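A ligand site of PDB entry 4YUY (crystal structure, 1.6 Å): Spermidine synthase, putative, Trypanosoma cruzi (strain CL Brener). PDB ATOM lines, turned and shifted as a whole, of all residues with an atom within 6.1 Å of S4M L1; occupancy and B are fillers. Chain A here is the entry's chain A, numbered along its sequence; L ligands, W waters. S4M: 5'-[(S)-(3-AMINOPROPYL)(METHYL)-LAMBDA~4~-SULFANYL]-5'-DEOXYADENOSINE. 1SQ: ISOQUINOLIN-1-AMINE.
Merely in contact with S4M L1: Leu 67, Gln 72, Tyr 81, Gly 103, Gly 104, Val 125, Asp 128, Val 131, Gly 156, Thr 177 and Leu 187.
Hydrophobic or aromatic side chains within 4 Å of S4M L1: Leu 67, Tyr 81, His 82, Ile 127, Val 131, Pro 183, Ala 184 and Leu 187.
22 residues have an atom within 4 Å of S4M L1: Gln 48, Leu 67, Gln 72, Tyr 81, His 82, Gly 103, Gly 104, Asp 106, Val 125, Asp 126, Ile 127, Asp 128, Val 131, Gly 156, Asp 157, Gly 158, Asp 176, Thr 177, Thr 178, Pro 183, Ala 184 and Leu 187.
A nitrogen (N7) of S4M L1 sits at hydrogen-bond distance from the backbone NH of Ala 184 (3.2 Å).
N1 of S4M L1 is in hydrogen-bond range of N of Gly 158 (2.9 Å).
N of S4M L1 lies within salt-bridge range of OD2 of Asp 106, at 2.7 Å.
A ring nitrogen (NE2) of His 82 lies within hydrogen-bond range of a nitrogen (N) of S4M L1, at 2.9 Å.
An oxygen (O2') of S4M L1 sits at hydrogen-bond distance from the side-chain carboxylate of Asp 126.
The backbone NH (N) of Thr 178 lies within hydrogen-bond range of an oxygen (O4') of S4M L1 (3.4 Å).
The side-chain carboxylate (OD2) of Asp 176 is in salt-bridge range of a nitrogen (N) of S4M L1 (2.8 Å).
The side-chain amide nitrogen (NE2) of Gln 48 sits at hydrogen-bond distance from an oxygen (O2') of S4M L1 (3.0 Å).
A nitrogen (N6) of S4M L1 is in hydrogen-bond range of the backbone carbonyl oxygen (O) of Pro 183 (3.0 Å).
A nitrogen (N6) of S4M L1 sits at hydrogen-bond distance from the side-chain carboxylate of Asp 157 (2.7 Å).
The backbone NH of Ile 127 lies within hydrogen-bond range of a nitrogen (N3) of S4M L1, at 3.2 Å.
Water W1 lies within hydrogen-bond range of OD2 of Asp 176 (2.6 Å), OD1 of Asp 106 (2.7 Å), N of Val 109 (2.9 Å), N of S4M L1 (3.2 Å) and N of Gly 108 (3.2 Å).
The backbone NH (N) of Asp 128 lies within hydrogen-bond range of the side-chain carboxylate (OD1) of Asp 126.
The backbone carbonyl oxygen (O) of Asp 126 lies within hydrogen-bond range of the backbone NH (N) of Gly 156 (3.0 Å).
The backbone NH of Gly 108 lies within hydrogen-bond range of the side-chain carboxylate of Asp 106, 2.9 Å away.
The side-chain carboxylate (OD2) of Asp 128 is in hydrogen-bond range of the side-chain amide nitrogen (NE2) of Gln 48, 2.9 Å away.
The backbone NH of Asp 176 lies within hydrogen-bond range of the backbone carbonyl oxygen of Ile 102 (2.7 Å).
OH of Tyr 81 lies within hydrogen-bond range of OD1 of Asp 176.
N of Gly 105 lies within hydrogen-bond range of OD2 of Asp 126 (2.9 Å).
O of Val 125 sits at hydrogen-bond distance from N of Gly 103 (2.8 Å).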
ATOM      1  N   GLN A  48      -2.052  11.313   5.179  1.00  0.00           N
ATOM      2  CA  GLN A  48      -2.813  11.646   3.970  1.00  0.00           C
ATOM      3  C   GLN A  48      -1.936  11.683   2.815  1.00  0.00           C
ATOM      4  O   GLN A  48      -0.681  11.735   2.977  1.00  0.00           O
ATOM      5  CB  GLN A  48      -3.515  13.037   4.126  1.00  0.00           C
ATOM      6  CG  GLN A  48      -4.518  13.045   5.304  1.00  0.00           C
ATOM      7  CD  GLN A  48      -4.941  14.455   5.732  1.00  0.00           C
ATOM      8  OE1 GLN A  48      -6.112  14.824   5.546  1.00  0.00           O
ATOM      9  NE2 GLN A  48      -3.999  15.241   6.292  1.00  0.00           N
ATOM     10  N   MET A  65      -3.477  22.969  -3.582  1.00  0.00           N
ATOM     11  CA  MET A  65      -3.124  21.920  -2.593  1.00  0.00           C
ATOM     12  C   MET A  65      -4.304  20.944  -2.559  1.00  0.00           C
ATOM     13  O   MET A  65      -5.428  21.393  -2.447  1.00  0.00           O
ATOM     14  CB  MET A  65      -2.888  22.485  -1.200  1.00  0.00           C
ATOM     15  CG  MET A  65      -2.763  21.355  -0.160  1.00  0.00           C
ATOM     16  SD  MET A  65      -2.886  21.919   1.574  1.00  0.00           S
ATOM     17  CE  MET A  65      -1.316  22.669   1.472  1.00  0.00           C
ATOM     18  N   LEU A  67      -5.536  17.116  -0.601  1.00  0.00           N
ATOM     19  CA  LEU A  67      -5.322  16.091   0.468  1.00  0.00           C
ATOM     20  C   LEU A  67      -6.226  14.901   0.177  1.00  0.00           C
ATOM     21  O   LEU A  67      -7.410  15.062  -0.033  1.00  0.00           O
ATOM     22  CB  LEU A  67      -5.637  16.651   1.858  1.00  0.00           C
ATOM     23  CG  LEU A  67      -4.505  17.485   2.478  1.00  0.00           C
ATOM     24  CD1 LEU A  67      -5.100  18.119   3.757  1.00  0.00           C
ATOM     25  CD2 LEU A  67      -3.379  16.596   2.800  1.00  0.00           C
ATOM     26  N   GLN A  72      -8.015  21.433  -1.551  1.00  0.00           N
ATOM     27  CA  GLN A  72      -8.167  22.075  -0.247  1.00  0.00           C
ATOM     28  C   GLN A  72      -8.107  23.542  -0.316  1.00  0.00           C
ATOM     29  O   GLN A  72      -8.897  24.245   0.373  1.00  0.00           O
ATOM     30  CB  GLN A  72      -7.064  21.607   0.764  1.00  0.00           C
ATOM     31  CG  GLN A  72      -7.061  20.097   0.887  1.00  0.00           C
ATOM     32  CD  GLN A  72      -8.263  19.616   1.672  1.00  0.00           C
ATOM     33  OE1 GLN A  72      -8.497  20.075   2.792  1.00  0.00           O
ATOM     34  NE2 GLN A  72      -8.967  18.658   1.132  1.00  0.00           N
ATOM     35  N   VAL A  73      -7.109  24.044  -1.027  1.00  0.00           N
ATOM     36  CA  VAL A  73      -6.966  25.480  -1.233  1.00  0.00           C
ATOM     37  C   VAL A  73      -6.439  25.780  -2.630  1.00  0.00           C
ATOM     38  O   VAL A  73      -5.779  24.954  -3.220  1.00  0.00           O
ATOM     39  CB  VAL A  73      -6.041  26.160  -0.209  1.00  0.00           C
ATOM     40  CG1 VAL A  73      -6.581  26.102   1.235  1.00  0.00           C
ATOM     41  CG2 VAL A  73      -4.648  25.547  -0.150  1.00  0.00           C
ATOM     42  N   TYR A  81     -13.679  30.900   2.023  1.00  0.00           N
ATOM     43  CA  TYR A  81     -13.962  29.990   3.164  1.00  0.00           C
ATOM     44  C   TYR A  81     -13.210  30.475   4.434  1.00  0.00           C
ATOM     45  O   TYR A  81     -13.767  30.359   5.561  1.00  0.00           O
ATOM     46  CB  TYR A  81     -13.735  28.514   2.738  1.00  0.00           C
ATOM     47  CG  TYR A  81     -13.656  27.528   3.852  1.00  0.00           C
ATOM     48  CD1 TYR A  81     -12.470  27.371   4.596  1.00  0.00           C
ATOM     49  CD2 TYR A  81     -14.734  26.696   4.110  1.00  0.00           C
ATOM     50  CE1 TYR A  81     -12.376  26.399   5.554  1.00  0.00           C
ATOM     51  CE2 TYR A  81     -14.662  25.703   5.076  1.00  0.00           C
ATOM     52  CZ  TYR A  81     -13.473  25.528   5.762  1.00  0.00           C
ATOM     53  OH  TYR A  81     -13.298  24.519   6.742  1.00  0.00           O
ATOM     54  N   HIS A  82     -11.967  30.974   4.313  1.00  0.00           N
ATOM     55  CA  HIS A  82     -11.215  31.440   5.485  1.00  0.00           C
ATOM     56  C   HIS A  82     -11.915  32.647   6.095  1.00  0.00           C
ATOM     57  O   HIS A  82     -12.044  32.697   7.290  1.00  0.00           O
ATOM     58  CB  HIS A  82      -9.731  31.692   5.134  1.00  0.00           C
ATOM     59  CG  HIS A  82      -9.071  30.419   4.683  1.00  0.00           C
ATOM     60  ND1 HIS A  82      -8.098  30.342   3.726  1.00  0.00           N
ATOM     61  CD2 HIS A  82      -9.277  29.154   5.117  1.00  0.00           C
ATOM     62  CE1 HIS A  82      -7.739  29.075   3.545  1.00  0.00           C
ATOM     63  NE2 HIS A  82      -8.417  28.339   4.397  1.00  0.00           N
ATOM     64  N   ILE A 102      -9.602  23.464  15.029  1.00  0.00           N
ATOM     65  CA  ILE A 102      -9.282  22.046  14.859  1.00  0.00           C
ATOM     66  C   ILE A 102      -9.103  21.894  13.383  1.00  0.00           C
ATOM     67  O   ILE A 102      -9.909  22.349  12.559  1.00  0.00           O
ATOM     68  CB  ILE A 102     -10.452  21.175  15.436  1.00  0.00           C
ATOM     69  CG1 ILE A 102     -10.457  21.296  16.968  1.00  0.00           C
ATOM     70  CG2 ILE A 102     -10.233  19.732  14.972  1.00  0.00           C
ATOM     71  CD1 ILE A 102     -11.528  20.569  17.674  1.00  0.00           C
ATOM     72  N   GLY A 103      -7.999  21.240  12.999  1.00  0.00           N
ATOM     73  CA  GLY A 103      -7.644  21.254  11.559  1.00  0.00           C
ATOM     74  C   GLY A 103      -6.915  22.553  11.181  1.00  0.00           C
ATOM     75  O   GLY A 103      -6.112  23.060  11.961  1.00  0.00           O
ATOM     76  N   GLY A 104      -7.210  23.079   9.999  1.00  0.00           N
ATOM     77  CA  GLY A 104      -6.655  24.419   9.747  1.00  0.00           C
ATOM     78  C   GLY A 104      -5.207  24.563   9.541  1.00  0.00           C
ATOM     79  O   GLY A 104      -4.663  25.656   9.648  1.00  0.00           O
ATOM     80  N   GLY A 105      -4.531  23.471   9.156  1.00  0.00           N
ATOM     81  CA  GLY A 105      -3.062  23.493   9.222  1.00  0.00           C
ATOM     82  C   GLY A 105      -2.469  24.393   8.155  1.00  0.00           C
ATOM     83  O   GLY A 105      -1.265  24.725   8.285  1.00  0.00           O
ATOM     84  N   ASP A 106      -3.264  24.767   7.102  1.00  0.00           N
ATOM     85  CA  ASP A 106      -2.777  25.741   6.077  1.00  0.00           C
ATOM     86  C   ASP A 106      -2.613  27.116   6.675  1.00  0.00           C
ATOM     87  O   ASP A 106      -1.883  27.931   6.087  1.00  0.00           O
ATOM     88  CB  ASP A 106      -3.715  25.775   4.859  1.00  0.00           C
ATOM     89  CG  ASP A 106      -5.091  25.920   5.249  1.00  0.00           C
ATOM     90  OD1 ASP A 106      -5.494  26.937   5.738  1.00  0.00           O
ATOM     91  OD2 ASP A 106      -5.835  24.895   5.151  1.00  0.00           O
ATOM     92  N   GLY A 107      -3.328  27.445   7.762  1.00  0.00           N
ATOM     93  CA  GLY A 107      -3.160  28.752   8.405  1.00  0.00           C
ATOM     94  C   GLY A 107      -4.231  29.773   7.989  1.00  0.00           C
ATOM     95  O   GLY A 107      -4.278  30.903   8.565  1.00  0.00           O
ATOM     96  N   GLY A 108      -5.103  29.447   7.049  1.00  0.00           N
ATOM     97  CA  GLY A 108      -6.041  30.497   6.484  1.00  0.00           C
ATOM     98  C   GLY A 108      -7.071  30.976   7.475  1.00  0.00           C
ATOM     99  O   GLY A 108      -7.289  32.200   7.647  1.00  0.00           O
ATOM    100  N   VAL A 109      -7.776  30.025   8.149  1.00  0.00           N
ATOM    101  CA  VAL A 109      -8.739  30.460   9.176  1.00  0.00           C
ATOM    102  C   VAL A 109      -7.959  31.243  10.305  1.00  0.00           C
ATOM    103  O   VAL A 109      -8.441  32.272  10.814  1.00  0.00           O
ATOM    104  CB  VAL A 109      -9.480  29.241   9.784  1.00  0.00           C
ATOM    105  CG1 VAL A 109     -10.290  29.695  11.066  1.00  0.00           C
ATOM    106  CG2 VAL A 109     -10.390  28.605   8.755  1.00  0.00           C
ATOM    107  N   VAL A 125      -4.910  22.880  16.177  1.00  0.00           N
ATOM    108  CA  VAL A 125      -4.457  21.548  16.331  1.00  0.00           C
ATOM    109  C   VAL A 125      -4.778  20.814  15.053  1.00  0.00           C
ATOM    110  O   VAL A 125      -5.980  20.559  14.744  1.00  0.00           O
ATOM    111  CB  VAL A 125      -5.131  20.837  17.559  1.00  0.00           C
ATOM    112  CG1 VAL A 125      -4.516  19.427  17.716  1.00  0.00           C
ATOM    113  CG2 VAL A 125      -4.932  21.712  18.805  1.00  0.00           C
ATOM    114  N   ASP A 126      -3.768  20.368  14.333  1.00  0.00           N
ATOM    115  CA  ASP A 126      -4.010  19.669  13.114  1.00  0.00           C
ATOM    116  C   ASP A 126      -3.223  18.387  13.103  1.00  0.00           C
ATOM    117  O   ASP A 126      -2.138  18.382  13.566  1.00  0.00           O
ATOM    118  CB  ASP A 126      -3.525  20.543  11.917  1.00  0.00           C
ATOM    119  CG  ASP A 126      -3.980  19.963  10.574  1.00  0.00           C
ATOM    120  OD1 ASP A 126      -3.636  18.772  10.217  1.00  0.00           O
ATOM    121  OD2 ASP A 126      -4.667  20.670   9.721  1.00  0.00           O
ATOM    122  N   ILE A 127      -3.853  17.295  12.658  1.00  0.00           N
ATOM    123  CA  ILE A 127      -3.269  15.940  12.784  1.00  0.00           C
ATOM    124  C   ILE A 127      -2.006  15.791  11.969  1.00  0.00           C
ATOM    125  O   ILE A 127      -1.044  15.062  12.396  1.00  0.00           O
ATOM    126  CB  ILE A 127      -4.316  14.835  12.500  1.00  0.00           C
ATOM    127  CG1 ILE A 127      -3.820  13.436  12.999  1.00  0.00           C
ATOM    128  CG2 ILE A 127      -4.604  14.815  10.995  1.00  0.00           C
ATOM    129  CD1 ILE A 127      -5.013  12.485  12.789  1.00  0.00           C
ATOM    130  N   ASP A 128      -1.904  16.568  10.907  1.00  0.00           N
ATOM    131  CA  ASP A 128      -0.904  16.306   9.897  1.00  0.00           C
ATOM    132  C   ASP A 128       0.059  17.470   9.865  1.00  0.00           C
ATOM    133  O   ASP A 128      -0.198  18.438   9.155  1.00  0.00           O
ATOM    134  CB  ASP A 128      -1.581  16.139   8.510  1.00  0.00           C
ATOM    135  CG  ASP A 128      -0.636  15.450   7.525  1.00  0.00           C
ATOM    136  OD1 ASP A 128       0.609  15.662   7.626  1.00  0.00           O
ATOM    137  OD2 ASP A 128      -1.144  14.760   6.611  1.00  0.00           O
ATOM    138  N   VAL A 131       1.172  19.374   6.580  1.00  0.00           N
ATOM    139  CA  VAL A 131       0.307  20.403   5.959  1.00  0.00           C
ATOM    140  C   VAL A 131       0.842  21.745   6.390  1.00  0.00           C
ATOM    141  O   VAL A 131       0.971  22.642   5.586  1.00  0.00           O
ATOM    142  CB  VAL A 131      -1.145  20.241   6.383  1.00  0.00           C
ATOM    143  CG1 VAL A 131      -2.026  21.439   5.917  1.00  0.00           C
ATOM    144  CG2 VAL A 131      -1.696  18.953   5.765  1.00  0.00           C
ATOM    145  N   GLY A 156      -1.504  17.080  16.163  1.00  0.00           N
ATOM    146  CA  GLY A 156      -2.213  16.052  16.863  1.00  0.00           C
ATOM    147  C   GLY A 156      -3.647  15.907  16.421  1.00  0.00           C
ATOM    148  O   GLY A 156      -4.235  16.776  15.738  1.00  0.00           O
ATOM    149  N   ASP A 157      -4.242  14.786  16.833  1.00  0.00           N
ATOM    150  CA  ASP A 157      -5.603  14.571  16.495  1.00  0.00           C
ATOM    151  C   ASP A 157      -6.592  15.470  17.306  1.00  0.00           C
ATOM    152  O   ASP A 157      -6.414  15.617  18.471  1.00  0.00           O
ATOM    153  CB  ASP A 157      -5.957  13.099  16.729  1.00  0.00           C
ATOM    154  CG  ASP A 157      -7.432  12.866  16.717  1.00  0.00           C
ATOM    155  OD1 ASP A 157      -8.139  13.147  15.713  1.00  0.00           O
ATOM    156  OD2 ASP A 157      -7.903  12.426  17.789  1.00  0.00           O
ATOM    157  N   GLY A 158      -7.538  16.102  16.633  1.00  0.00           N
ATOM    158  CA  GLY A 158      -8.491  17.059  17.290  1.00  0.00           C
ATOM    159  C   GLY A 158      -9.343  16.387  18.339  1.00  0.00           C
ATOM    160  O   GLY A 158      -9.754  17.009  19.310  1.00  0.00           O
ATOM    161  N   LEU A 159      -9.670  15.122  18.118  1.00  0.00           N
ATOM    162  CA  LEU A 159     -10.593  14.427  19.055  1.00  0.00           C
ATOM    163  C   LEU A 159      -9.901  14.202  20.365  1.00  0.00           C
ATOM    164  O   LEU A 159     -10.403  14.545  21.396  1.00  0.00           O
ATOM    165  CB  LEU A 159     -11.097  13.101  18.465  1.00  0.00           C
ATOM    166  CG  LEU A 159     -12.103  12.381  19.388  1.00  0.00           C
ATOM    167  CD1 LEU A 159     -13.317  13.210  19.851  1.00  0.00           C
ATOM    168  CD2 LEU A 159     -12.501  11.083  18.704  1.00  0.00           C
ATOM    169  N   ASP A 176     -12.075  23.108  11.108  1.00  0.00           N
ATOM    170  CA  ASP A 176     -11.767  23.338   9.652  1.00  0.00           C
ATOM    171  C   ASP A 176     -11.093  22.070   9.145  1.00  0.00           C
ATOM    172  O   ASP A 176      -9.832  21.953   9.161  1.00  0.00           O
ATOM    173  CB  ASP A 176     -10.834  24.570   9.459  1.00  0.00           C
ATOM    174  CG  ASP A 176     -10.247  24.659   8.022  1.00  0.00           C
ATOM    175  OD1 ASP A 176     -10.770  24.026   7.132  1.00  0.00           O
ATOM    176  OD2 ASP A 176      -9.223  25.348   7.790  1.00  0.00           O
ATOM    177  N   THR A 177     -11.928  21.106   8.764  1.00  0.00           N
ATOM    178  CA  THR A 177     -11.426  19.763   8.476  1.00  0.00           C
ATOM    179  C   THR A 177     -11.558  19.400   7.046  1.00  0.00           C
ATOM    180  O   THR A 177     -12.279  20.046   6.289  1.00  0.00           O
ATOM    181  CB  THR A 177     -12.202  18.694   9.289  1.00  0.00           C
ATOM    182  OG1 THR A 177     -13.560  18.675   8.873  1.00  0.00           O
ATOM    183  CG2 THR A 177     -12.094  18.966  10.764  1.00  0.00           C
ATOM    184  N   THR A 178     -10.820  18.348   6.695  1.00  0.00           N
ATOM    185  CA  THR A 178     -11.061  17.655   5.447  1.00  0.00           C
ATOM    186  C   THR A 178     -12.463  16.974   5.488  1.00  0.00           C
ATOM    187  O   THR A 178     -13.210  17.021   6.492  1.00  0.00           O
ATOM    188  CB  THR A 178      -9.954  16.570   5.227  1.00  0.00           C
ATOM    189  OG1 THR A 178      -9.701  15.940   6.516  1.00  0.00           O
ATOM    190  CG2 THR A 178      -8.642  17.206   4.784  1.00  0.00           C
ATOM    191  N   GLY A 182     -11.285   9.724   5.646  1.00  0.00           N
ATOM    192  CA  GLY A 182      -9.924  10.020   6.075  1.00  0.00           C
ATOM    193  C   GLY A 182      -9.910  10.331   7.556  1.00  0.00           C
ATOM    194  O   GLY A 182     -10.831  10.009   8.274  1.00  0.00           O
ATOM    195  N   PRO A 183      -8.854  11.030   7.969  1.00  0.00           N
ATOM    196  CA  PRO A 183      -8.541  11.155   9.410  1.00  0.00           C
ATOM    197  C   PRO A 183      -9.559  12.052  10.081  1.00  0.00           C
ATOM    198  O   PRO A 183      -9.585  12.066  11.320  1.00  0.00           O
ATOM    199  CB  PRO A 183      -7.143  11.794   9.405  1.00  0.00           C
ATOM    200  CG  PRO A 183      -6.976  12.420   8.066  1.00  0.00           C
ATOM    201  CD  PRO A 183      -7.729  11.520   7.146  1.00  0.00           C
ATOM    202  N   ALA A 184     -10.374  12.793   9.310  1.00  0.00           N
ATOM    203  CA  ALA A 184     -11.413  13.633   9.980  1.00  0.00           C
ATOM    204  C   ALA A 184     -12.702  12.900  10.296  1.00  0.00           C
ATOM    205  O   ALA A 184     -13.638  13.511  10.828  1.00  0.00           O
ATOM    206  CB  ALA A 184     -11.791  14.814   9.087  1.00  0.00           C
ATOM    207  N   SER A 185     -12.740  11.629   9.986  1.00  0.00           N
ATOM    208  CA  SER A 185     -14.039  10.909  10.141  1.00  0.00           C
ATOM    209  C   SER A 185     -14.778  11.178  11.484  1.00  0.00           C
ATOM    210  O   SER A 185     -15.984  11.526  11.504  1.00  0.00           O
ATOM    211  CB  SER A 185     -13.776   9.409   9.922  1.00  0.00           C
ATOM    212  OG  SER A 185     -14.981   8.740  10.022  1.00  0.00           O
ATOM    213  N   LEU A 187     -14.540  13.534  13.455  1.00  0.00           N
ATOM    214  CA  LEU A 187     -14.842  14.984  13.704  1.00  0.00           C
ATOM    215  C   LEU A 187     -16.172  15.438  13.075  1.00  0.00           C
ATOM    216  O   LEU A 187     -16.620  16.581  13.257  1.00  0.00           O
ATOM    217  CB  LEU A 187     -13.672  15.882  13.237  1.00  0.00           C
ATOM    218  CG  LEU A 187     -12.302  15.482  13.765  1.00  0.00           C
ATOM    219  CD1 LEU A 187     -11.259  16.470  13.231  1.00  0.00           C
ATOM    220  CD2 LEU A 187     -12.311  15.502  15.253  1.00  0.00           C
HETATM  221  CA  S4M L   1      -9.190  24.978   4.066  1.00  0.00           C
HETATM  222  N   S4M L   1      -8.402  25.562   5.164  1.00  0.00           N
HETATM  223  CB  S4M L   1      -8.679  23.560   3.706  1.00  0.00           C
HETATM  224  CG  S4M L   1      -8.981  22.551   4.847  1.00  0.00           C
HETATM  225  SD  S4M L   1      -7.645  22.263   6.005  1.00  0.00           S
HETATM  226  CE  S4M L   1      -6.360  21.614   4.919  1.00  0.00           C
HETATM  227  C5' S4M L   1      -8.267  20.687   6.712  1.00  0.00           C
HETATM  228  C4' S4M L   1      -7.242  20.050   7.675  1.00  0.00           C
HETATM  229  O4' S4M L   1      -8.013  19.110   8.513  1.00  0.00           O
HETATM  230  C1' S4M L   1      -6.965  18.308   9.087  1.00  0.00           C
HETATM  231  C2' S4M L   1      -6.202  17.875   7.848  1.00  0.00           C
HETATM  232  O2' S4M L   1      -4.869  17.421   8.178  1.00  0.00           O
HETATM  233  C3' S4M L   1      -6.176  19.169   7.011  1.00  0.00           C
HETATM  234  O3' S4M L   1      -4.954  19.931   7.069  1.00  0.00           O
HETATM  235  N9  S4M L   1      -7.498  17.155   9.835  1.00  0.00           N
HETATM  236  C8  S4M L   1      -8.068  16.005   9.308  1.00  0.00           C
HETATM  237  N7  S4M L   1      -8.401  15.149  10.268  1.00  0.00           N
HETATM  238  C5  S4M L   1      -8.034  15.759  11.442  1.00  0.00           C
HETATM  239  C6  S4M L   1      -8.058  15.345  12.774  1.00  0.00           C
HETATM  240  N6  S4M L   1      -8.583  14.145  13.237  1.00  0.00           N
HETATM  241  C4  S4M L   1      -7.443  17.002  11.206  1.00  0.00           C
HETATM  242  N3  S4M L   1      -6.960  17.861  12.115  1.00  0.00           N
HETATM  243  C2  S4M L   1      -7.067  17.411  13.363  1.00  0.00           C
HETATM  244  N1  S4M L   1      -7.609  16.203  13.689  1.00  0.00           N
HETATM  245  N1  1SQ L   2     -11.805  23.153  -1.426  1.00  0.00           N
HETATM  246  C2  1SQ L   2     -12.046  23.744  -0.212  1.00  0.00           C
HETATM  247  N3  1SQ L   2     -12.176  25.073  -0.292  1.00  0.00           N
HETATM  248  C4  1SQ L   2     -12.416  25.670   0.892  1.00  0.00           C
HETATM  249  C5  1SQ L   2     -12.499  25.013   2.094  1.00  0.00           C
HETATM  250  C6  1SQ L   2     -12.346  23.633   2.127  1.00  0.00           C
HETATM  251  C7  1SQ L   2     -12.412  22.905   3.305  1.00  0.00           C
HETATM  252  C8  1SQ L   2     -12.247  21.537   3.269  1.00  0.00           C
HETATM  253  C9  1SQ L   2     -12.033  20.875   2.088  1.00  0.00           C
HETATM  254  C10 1SQ L   2     -11.958  21.611   0.929  1.00  0.00           C
HETATM  255  C11 1SQ L   2     -12.098  22.987   0.940  1.00  0.00           C
HETATM  256  O   HOH W   1      -7.373  27.222   7.659  1.00  0.00           O
